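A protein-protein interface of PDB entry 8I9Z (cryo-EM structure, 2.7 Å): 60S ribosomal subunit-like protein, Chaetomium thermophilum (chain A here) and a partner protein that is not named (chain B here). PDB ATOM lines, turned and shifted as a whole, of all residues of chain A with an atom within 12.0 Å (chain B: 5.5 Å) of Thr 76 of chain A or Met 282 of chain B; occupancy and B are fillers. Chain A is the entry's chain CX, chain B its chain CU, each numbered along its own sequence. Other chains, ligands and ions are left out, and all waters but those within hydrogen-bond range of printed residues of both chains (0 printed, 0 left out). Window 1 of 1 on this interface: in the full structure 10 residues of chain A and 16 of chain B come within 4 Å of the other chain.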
ATOM      1  N   GLU A  66       0.537   8.609  10.563  1.00  0.00           N
ATOM      2  CA  GLU A  66      -0.192   8.993  11.768  1.00  0.00           C
ATOM      3  C   GLU A  66      -0.018   7.968  12.880  1.00  0.00           C
ATOM      4  O   GLU A  66      -0.169   8.312  14.057  1.00  0.00           O
ATOM      5  CB  GLU A  66      -1.669   9.207  11.394  1.00  0.00           C
ATOM      6  CG  GLU A  66      -2.644   9.693  12.483  1.00  0.00           C
ATOM      7  CD  GLU A  66      -3.131   8.589  13.411  1.00  0.00           C
ATOM      8  OE1 GLU A  66      -3.217   7.428  12.960  1.00  0.00           O
ATOM      9  OE2 GLU A  66      -3.428   8.884  14.587  1.00  0.00           O
ATOM     10  N   ILE A  71      -1.080  10.862  17.910  1.00  0.00           N
ATOM     11  CA  ILE A  71      -2.263  11.657  17.593  1.00  0.00           C
ATOM     12  C   ILE A  71      -3.458  11.062  18.326  1.00  0.00           C
ATOM     13  O   ILE A  71      -3.716   9.858  18.187  1.00  0.00           O
ATOM     14  CB  ILE A  71      -2.525  11.705  16.080  1.00  0.00           C
ATOM     15  CG1 ILE A  71      -1.318  12.294  15.354  1.00  0.00           C
ATOM     16  CG2 ILE A  71      -3.766  12.520  15.782  1.00  0.00           C
ATOM     17  CD1 ILE A  71      -0.964  13.686  15.807  1.00  0.00           C
ATOM     18  N   PRO A  72      -4.188  11.847  19.114  1.00  0.00           N
ATOM     19  CA  PRO A  72      -5.388  11.324  19.773  1.00  0.00           C
ATOM     20  C   PRO A  72      -6.490  11.024  18.772  1.00  0.00           C
ATOM     21  O   PRO A  72      -6.564  11.616  17.695  1.00  0.00           O
ATOM     22  CB  PRO A  72      -5.800  12.461  20.716  1.00  0.00           C
ATOM     23  CG  PRO A  72      -4.602  13.357  20.803  1.00  0.00           C
ATOM     24  CD  PRO A  72      -3.924  13.244  19.486  1.00  0.00           C
ATOM     25  N   GLN A  73      -7.351  10.082  19.141  1.00  0.00           N
ATOM     26  CA  GLN A  73      -8.504   9.752  18.319  1.00  0.00           C
ATOM     27  C   GLN A  73      -9.609  10.775  18.532  1.00  0.00           C
ATOM     28  O   GLN A  73      -9.880  11.191  19.661  1.00  0.00           O
ATOM     29  CB  GLN A  73      -9.012   8.349  18.646  1.00  0.00           C
ATOM     30  CG  GLN A  73      -7.922   7.378  19.041  1.00  0.00           C
ATOM     31  CD  GLN A  73      -8.284   5.945  18.724  1.00  0.00           C
ATOM     32  OE1 GLN A  73      -8.210   5.515  17.575  1.00  0.00           O
ATOM     33  NE2 GLN A  73      -8.673   5.194  19.744  1.00  0.00           N
ATOM     34  N   LEU A  74     -10.251  11.175  17.441  1.00  0.00           N
ATOM     35  CA  LEU A  74     -11.221  12.259  17.451  1.00  0.00           C
ATOM     36  C   LEU A  74     -12.612  11.724  17.152  1.00  0.00           C
ATOM     37  O   LEU A  74     -12.792  10.907  16.244  1.00  0.00           O
ATOM     38  CB  LEU A  74     -10.846  13.333  16.432  1.00  0.00           C
ATOM     39  CG  LEU A  74      -9.547  14.078  16.736  1.00  0.00           C
ATOM     40  CD1 LEU A  74      -9.149  14.934  15.558  1.00  0.00           C
ATOM     41  CD2 LEU A  74      -9.688  14.922  17.986  1.00  0.00           C
ATOM     42  N   ASN A  75     -13.597  12.196  17.913  1.00  0.00           N
ATOM     43  CA  ASN A  75     -14.976  11.733  17.776  1.00  0.00           C
ATOM     44  C   ASN A  75     -15.604  12.425  16.575  1.00  0.00           C
ATOM     45  O   ASN A  75     -15.639  13.652  16.492  1.00  0.00           O
ATOM     46  CB  ASN A  75     -15.764  11.997  19.051  1.00  0.00           C
ATOM     47  CG  ASN A  75     -17.006  11.143  19.150  1.00  0.00           C
ATOM     48  OD1 ASN A  75     -17.276  10.319  18.281  1.00  0.00           O
ATOM     49  ND2 ASN A  75     -17.771  11.332  20.216  1.00  0.00           N
ATOM     50  N   THR A  76     -16.083  11.629  15.637  1.00  0.00           N
ATOM     51  CA  THR A  76     -16.651  12.064  14.376  1.00  0.00           C
ATOM     52  C   THR A  76     -17.995  11.321  14.256  1.00  0.00           C
ATOM     53  O   THR A  76     -18.378  10.589  15.174  1.00  0.00           O
ATOM     54  CB  THR A  76     -15.546  11.830  13.312  1.00  0.00           C
ATOM     55  OG1 THR A  76     -14.597  12.901  13.393  1.00  0.00           O
ATOM     56  CG2 THR A  76     -15.996  11.755  11.850  1.00  0.00           C
ATOM     57  N   VAL A  77     -18.760  11.569  13.184  1.00  0.00           N
ATOM     58  CA  VAL A  77     -19.926  10.757  12.831  1.00  0.00           C
ATOM     59  C   VAL A  77     -19.606   9.267  12.891  1.00  0.00           C
ATOM     60  O   VAL A  77     -20.414   8.469  13.382  1.00  0.00           O
ATOM     61  CB  VAL A  77     -20.442  11.183  11.437  1.00  0.00           C
ATOM     62  CG1 VAL A  77     -21.422  10.178  10.868  1.00  0.00           C
ATOM     63  CG2 VAL A  77     -21.077  12.556  11.509  1.00  0.00           C
ATOM     64  N   THR A  78     -18.418   8.872  12.445  1.00  0.00           N
ATOM     65  CA  THR A  78     -17.884   7.564  12.805  1.00  0.00           C
ATOM     66  C   THR A  78     -17.434   7.595  14.261  1.00  0.00           C
ATOM     67  O   THR A  78     -16.543   8.379  14.604  1.00  0.00           O
ATOM     68  CB  THR A  78     -16.716   7.189  11.908  1.00  0.00           C
ATOM     69  OG1 THR A  78     -17.146   7.177  10.544  1.00  0.00           O
ATOM     70  CG2 THR A  78     -16.200   5.812  12.272  1.00  0.00           C
ATOM     71  N   PRO A  79     -18.008   6.776  15.137  1.00  0.00           N
ATOM     72  CA  PRO A  79     -17.693   6.881  16.566  1.00  0.00           C
ATOM     73  C   PRO A  79     -16.308   6.360  16.907  1.00  0.00           C
ATOM     74  O   PRO A  79     -15.741   5.517  16.207  1.00  0.00           O
ATOM     75  CB  PRO A  79     -18.779   6.029  17.229  1.00  0.00           C
ATOM     76  CG  PRO A  79     -19.227   5.113  16.180  1.00  0.00           C
ATOM     77  CD  PRO A  79     -19.090   5.816  14.879  1.00  0.00           C
ATOM     78  N   VAL A  80     -15.767   6.876  18.011  1.00  0.00           N
ATOM     79  CA  VAL A  80     -14.468   6.412  18.481  1.00  0.00           C
ATOM     80  C   VAL A  80     -14.582   5.076  19.195  1.00  0.00           C
ATOM     81  O   VAL A  80     -13.677   4.241  19.096  1.00  0.00           O
ATOM     82  CB  VAL A  80     -13.804   7.466  19.383  1.00  0.00           C
ATOM     83  CG1 VAL A  80     -13.223   8.570  18.548  1.00  0.00           C
ATOM     84  CG2 VAL A  80     -14.810   8.036  20.364  1.00  0.00           C
ATOM     85  N   GLY A  81     -15.670   4.847  19.919  1.00  0.00           N
ATOM     86  CA  GLY A  81     -15.783   3.642  20.698  1.00  0.00           C
ATOM     87  C   GLY A  81     -14.891   3.704  21.927  1.00  0.00           C
ATOM     88  O   GLY A  81     -14.331   4.743  22.281  1.00  0.00           O
ATOM     89  N   VAL A  82     -14.764   2.558  22.581  1.00  0.00           N
ATOM     90  CA  VAL A  82     -13.889   2.442  23.740  1.00  0.00           C
ATOM     91  C   VAL A  82     -12.455   2.334  23.251  1.00  0.00           C
ATOM     92  O   VAL A  82     -12.129   1.469  22.432  1.00  0.00           O
ATOM     93  CB  VAL A  82     -14.282   1.232  24.600  1.00  0.00           C
ATOM     94  CG1 VAL A  82     -13.770   1.404  26.018  1.00  0.00           C
ATOM     95  CG2 VAL A  82     -15.787   1.053  24.596  1.00  0.00           C
ATOM     96  N   THR A  83     -11.594   3.213  23.747  1.00  0.00           N
ATOM     97  CA  THR A  83     -10.218   3.309  23.284  1.00  0.00           C
ATOM     98  C   THR A  83      -9.307   2.563  24.249  1.00  0.00           C
ATOM     99  O   THR A  83      -9.323   2.827  25.454  1.00  0.00           O
ATOM    100  CB  THR A  83      -9.784   4.768  23.162  1.00  0.00           C
ATOM    101  OG1 THR A  83      -9.662   5.341  24.468  1.00  0.00           O
ATOM    102  CG2 THR A  83     -10.809   5.558  22.368  1.00  0.00           C
ATOM    103  N   ARG B 267     -22.226   4.855  23.364  1.00  0.00           N
ATOM    104  CA  ARG B 267     -22.582   4.951  21.960  1.00  0.00           C
ATOM    105  C   ARG B 267     -22.069   3.726  21.217  1.00  0.00           C
ATOM    106  O   ARG B 267     -20.877   3.411  21.314  1.00  0.00           O
ATOM    107  CB  ARG B 267     -22.007   6.226  21.355  1.00  0.00           C
ATOM    108  CG  ARG B 267     -22.374   6.448  19.904  1.00  0.00           C
ATOM    109  CD  ARG B 267     -21.507   7.519  19.282  1.00  0.00           C
ATOM    110  NE  ARG B 267     -22.099   8.031  18.054  1.00  0.00           N
ATOM    111  CZ  ARG B 267     -21.444   8.723  17.132  1.00  0.00           C
ATOM    112  NH1 ARG B 267     -20.180   9.065  17.296  1.00  0.00           N
ATOM    113  NH2 ARG B 267     -22.079   9.088  16.024  1.00  0.00           N
ATOM    114  N   MET B 275     -23.470  15.438  14.676  1.00  0.00           N
ATOM    115  CA  MET B 275     -22.739  15.881  15.851  1.00  0.00           C
ATOM    116  C   MET B 275     -22.730  17.404  15.904  1.00  0.00           C
ATOM    117  O   MET B 275     -23.118  18.081  14.950  1.00  0.00           O
ATOM    118  CB  MET B 275     -21.315  15.318  15.849  1.00  0.00           C
ATOM    119  CG  MET B 275     -21.262  13.830  15.559  1.00  0.00           C
ATOM    120  SD  MET B 275     -20.837  12.860  17.010  1.00  0.00           S
ATOM    121  CE  MET B 275     -19.089  13.184  17.134  1.00  0.00           C
ATOM    122  N   ARG B 277     -20.146  19.404  16.150  1.00  0.00           N
ATOM    123  CA  ARG B 277     -19.106  19.910  15.269  1.00  0.00           C
ATOM    124  C   ARG B 277     -19.014  19.019  14.043  1.00  0.00           C
ATOM    125  O   ARG B 277     -19.012  17.791  14.155  1.00  0.00           O
ATOM    126  CB  ARG B 277     -17.764  19.962  15.991  1.00  0.00           C
ATOM    127  CG  ARG B 277     -17.847  20.611  17.350  1.00  0.00           C
ATOM    128  CD  ARG B 277     -16.549  20.488  18.101  1.00  0.00           C
ATOM    129  NE  ARG B 277     -15.479  21.268  17.500  1.00  0.00           N
ATOM    130  CZ  ARG B 277     -14.236  21.297  17.955  1.00  0.00           C
ATOM    131  NH1 ARG B 277     -13.868  20.581  19.002  1.00  0.00           N
ATOM    132  NH2 ARG B 277     -13.338  22.059  17.341  1.00  0.00           N
ATOM    133  N   THR B 278     -18.944  19.644  12.873  1.00  0.00           N
ATOM    134  CA  THR B 278     -19.018  18.922  11.616  1.00  0.00           C
ATOM    135  C   THR B 278     -17.745  18.115  11.377  1.00  0.00           C
ATOM    136  O   THR B 278     -16.713  18.320  12.020  1.00  0.00           O
ATOM    137  CB  THR B 278     -19.260  19.891  10.462  1.00  0.00           C
ATOM    138  OG1 THR B 278     -18.130  20.758  10.322  1.00  0.00           O
ATOM    139  CG2 THR B 278     -20.494  20.727  10.729  1.00  0.00           C
ATOM    140  N   ASP B 279     -17.840  17.170  10.436  1.00  0.00           N
ATOM    141  CA  ASP B 279     -16.676  16.378  10.052  1.00  0.00           C
ATOM    142  C   ASP B 279     -15.627  17.245   9.374  1.00  0.00           C
ATOM    143  O   ASP B 279     -14.431  16.942   9.427  1.00  0.00           O
ATOM    144  CB  ASP B 279     -17.095  15.235   9.132  1.00  0.00           C
ATOM    145  CG  ASP B 279     -17.789  14.116   9.872  1.00  0.00           C
ATOM    146  OD1 ASP B 279     -18.245  14.348  11.011  1.00  0.00           O
ATOM    147  OD2 ASP B 279     -17.880  13.004   9.316  1.00  0.00           O
ATOM    148  N   ALA B 280     -16.063  18.318   8.710  1.00  0.00           N
ATOM    149  CA  ALA B 280     -15.122  19.276   8.148  1.00  0.00           C
ATOM    150  C   ALA B 280     -14.326  19.970   9.244  1.00  0.00           C
ATOM    151  O   ALA B 280     -13.119  20.184   9.097  1.00  0.00           O
ATOM    152  CB  ALA B 280     -15.864  20.298   7.289  1.00  0.00           C
ATOM    153  N   THR B 281     -14.981  20.323  10.352  1.00  0.00           N
ATOM    154  CA  THR B 281     -14.281  20.954  11.469  1.00  0.00           C
ATOM    155  C   THR B 281     -13.338  19.973  12.155  1.00  0.00           C
ATOM    156  O   THR B 281     -12.214  20.337  12.521  1.00  0.00           O
ATOM    157  CB  THR B 281     -15.289  21.521  12.467  1.00  0.00           C
ATOM    158  OG1 THR B 281     -16.176  22.414  11.785  1.00  0.00           O
ATOM    159  CG2 THR B 281     -14.590  22.275  13.585  1.00  0.00           C
ATOM    160  N   MET B 282     -13.775  18.725  12.327  1.00  0.00           N
ATOM    161  CA  MET B 282     -12.922  17.681  12.885  1.00  0.00           C
ATOM    162  C   MET B 282     -11.721  17.374  12.005  1.00  0.00           C
ATOM    163  O   MET B 282     -10.697  16.906  12.512  1.00  0.00           O
ATOM    164  CB  MET B 282     -13.737  16.406  13.110  1.00  0.00           C
ATOM    165  CG  MET B 282     -14.836  16.424  14.189  1.00  0.00           C
ATOM    166  SD  MET B 282     -14.342  16.600  15.926  1.00  0.00           S
ATOM    167  CE  MET B 282     -14.069  18.344  16.166  1.00  0.00           C
ATOM    168  N   GLU B 283     -11.828  17.610  10.698  1.00  0.00           N
ATOM    169  CA  GLU B 283     -10.683  17.404   9.820  1.00  0.00           C
ATOM    170  C   GLU B 283      -9.602  18.443  10.074  1.00  0.00           C
ATOM    171  O   GLU B 283      -8.412  18.116  10.087  1.00  0.00           O
ATOM    172  CB  GLU B 283     -11.131  17.431   8.363  1.00  0.00           C
ATOM    173  CG  GLU B 283     -10.941  16.108   7.649  1.00  0.00           C
ATOM    174  CD  GLU B 283      -9.482  15.728   7.495  1.00  0.00           C
ATOM    175  OE1 GLU B 283      -8.645  16.635   7.302  1.00  0.00           O
ATOM    176  OE2 GLU B 283      -9.167  14.523   7.574  1.00  0.00           O
ATOM    177  N   LYS B 284      -9.994  19.699  10.293  1.00  0.00           N
ATOM    178  CA  LYS B 284      -9.014  20.741  10.576  1.00  0.00           C
ATOM    179  C   LYS B 284      -8.388  20.559  11.952  1.00  0.00           C
ATOM    180  O   LYS B 284      -7.246  20.975  12.181  1.00  0.00           O
ATOM    181  CB  LYS B 284      -9.662  22.118  10.455  1.00  0.00           C
ATOM    182  CG  LYS B 284     -10.676  22.217   9.347  1.00  0.00           C
ATOM    183  CD  LYS B 284     -10.545  23.516   8.587  1.00  0.00           C
ATOM    184  CE  LYS B 284     -11.391  24.601   9.223  1.00  0.00           C
ATOM    185  NZ  LYS B 284     -12.830  24.446   8.887  1.00  0.00           N
ATOM    186  N   VAL B 285      -9.125  19.956  12.885  1.00  0.00           N
ATOM    187  CA  VAL B 285      -8.563  19.633  14.192  1.00  0.00           C
ATOM    188  C   VAL B 285      -7.490  18.562  14.052  1.00  0.00           C
ATOM    189  O   VAL B 285      -6.417  18.645  14.663  1.00  0.00           O
ATOM    190  CB  VAL B 285      -9.680  19.199  15.160  1.00  0.00           C
ATOM    191  CG1 VAL B 285      -9.102  18.652  16.451  1.00  0.00           C
ATOM    192  CG2 VAL B 285     -10.608  20.361  15.446  1.00  0.00           C
ATOM    193  N   LYS B 286      -7.758  17.546  13.230  1.00  0.00           N
ATOM    194  CA  LYS B 286      -6.786  16.474  13.033  1.00  0.00           C
ATOM    195  C   LYS B 286      -5.567  16.956  12.258  1.00  0.00           C
ATOM    196  O   LYS B 286      -4.440  16.552  12.558  1.00  0.00           O
ATOM    197  CB  LYS B 286      -7.437  15.295  12.318  1.00  0.00           C
ATOM    198  CG  LYS B 286      -6.863  13.949  12.713  1.00  0.00           C
ATOM    199  CD  LYS B 286      -7.444  12.835  11.865  1.00  0.00           C
ATOM    200  CE  LYS B 286      -6.467  12.388  10.792  1.00  0.00           C
ATOM    201  NZ  LYS B 286      -5.102  12.158  11.342  1.00  0.00           N
ATOM    202  N   GLN B 287      -5.769  17.811  11.253  1.00  0.00           N
ATOM    203  CA  GLN B 287      -4.635  18.315  10.485  1.00  0.00           C
ATOM    204  C   GLN B 287      -3.780  19.262  11.313  1.00  0.00           C
ATOM    205  O   GLN B 287      -2.567  19.359  11.096  1.00  0.00           O
ATOM    206  CB  GLN B 287      -5.116  19.005   9.210  1.00  0.00           C
ATOM    207  CG  GLN B 287      -5.810  18.090   8.214  1.00  0.00           C
ATOM    208  CD  GLN B 287      -4.939  16.939   7.735  1.00  0.00           C
ATOM    209  OE1 GLN B 287      -3.714  17.052   7.661  1.00  0.00           O
ATOM    210  NE2 GLN B 287      -5.574  15.822   7.404  1.00  0.00           N
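The side-chain amide oxygen (OD1) of Asn 75 of chain A sits at hydrogen-bond distance from the guanidinium group (NH1) of Arg 267 of chain B.
The guanidinium group (NH1) of Arg 267 of chain B lies within hydrogen-bond range of the backbone carbonyl oxygen (O) of Thr 76 of chain A (3.2 Å).
NH2 of Arg 267 of chain B sits at hydrogen-bond distance from O of Val 77 of chain A.
O of Asn 75 of chain A lies close to SD of Met 282 of chain B (3.3 Å).
Lys 286 of chain B touches Glu 66 of chain A.
Met 282 of chain B touches Leu 74 of chain A.
Leu 74 of chain A touches Val 285 of chain B.
Lys 286 of chain B touches Leu 74 of chain A.
Met 275 of chain B touches Asn 75 of chain A (CE to O, 3.5 Å).
Thr 76 of chain A touches Met 275 of chain B.
Thr 76 of chain A touches Asp 279 of chain B.
Thr 76 of chain A touches Met 282 of chain B.
CG2 of Val 77 of chain A touches OD1 of Asp 279 of chain B, 3.4 Å away.
NH1 of Arg 267 of chain B touches CB of Pro 79 of chain A, 3.3 Å away.
Met 282 of chain B touches three residues of chain A.
No residue of chain A comes within 4 Å of Arg 277 of chain B.
No residue of chain A comes within 4 Å of Thr 278 of chain B.
Asp 279 of chain B touches just these residues of chain A: Thr 76 (3.4 Å) and Val 77 (3.4 Å).
Ala 280 of chain B touches none of the printed residues of chain A.
No residue of chain A comes within 4 Å of Glu 283 of chain B.
No residue of chain A comes within 4 Å of Lys 284 of chain B.
Of chain A, only Leu 74 comes within 4 Å of Val 285 of chain B.
Lys 286 of chain B touches two residues of chain A.
Of the printed residues of chain B, Val 77 of chain A touches Arg 267 and Asp 279.
Of the printed residues of chain B, Asn 75 of chain A touches Arg 267 (3.3 Å), Met 275 (3.5 Å) and Met 282 (3.3 Å).
Printed residues of chain B within 4 Å of Glu 66 of chain A: Lys 286.
Thr 78 of chain A touches none of the printed residues of chain B.
Val 82 of chain A touches none of the printed residues of chain B.
The nearest printed residue of chain A that does not touch Met 275 of chain B is Val 77 of chain A (4.1 Å).
Hydrophobic or aromatic side chains of chain B within 4 Å of the printed part of chain A: Met 275, Met 282 and Val 285.
Printed residues of chain A that touch a printed residue of chain B: Glu 66, Leu 74, Asn 75, Thr 76, Val 77 and Pro 79.
Hydrophobic or aromatic side chains of chain A that line the printed part of chain B: Leu 74, Val 77 and Pro 79.
Among the printed residues, 14 pairs touch across the chains.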
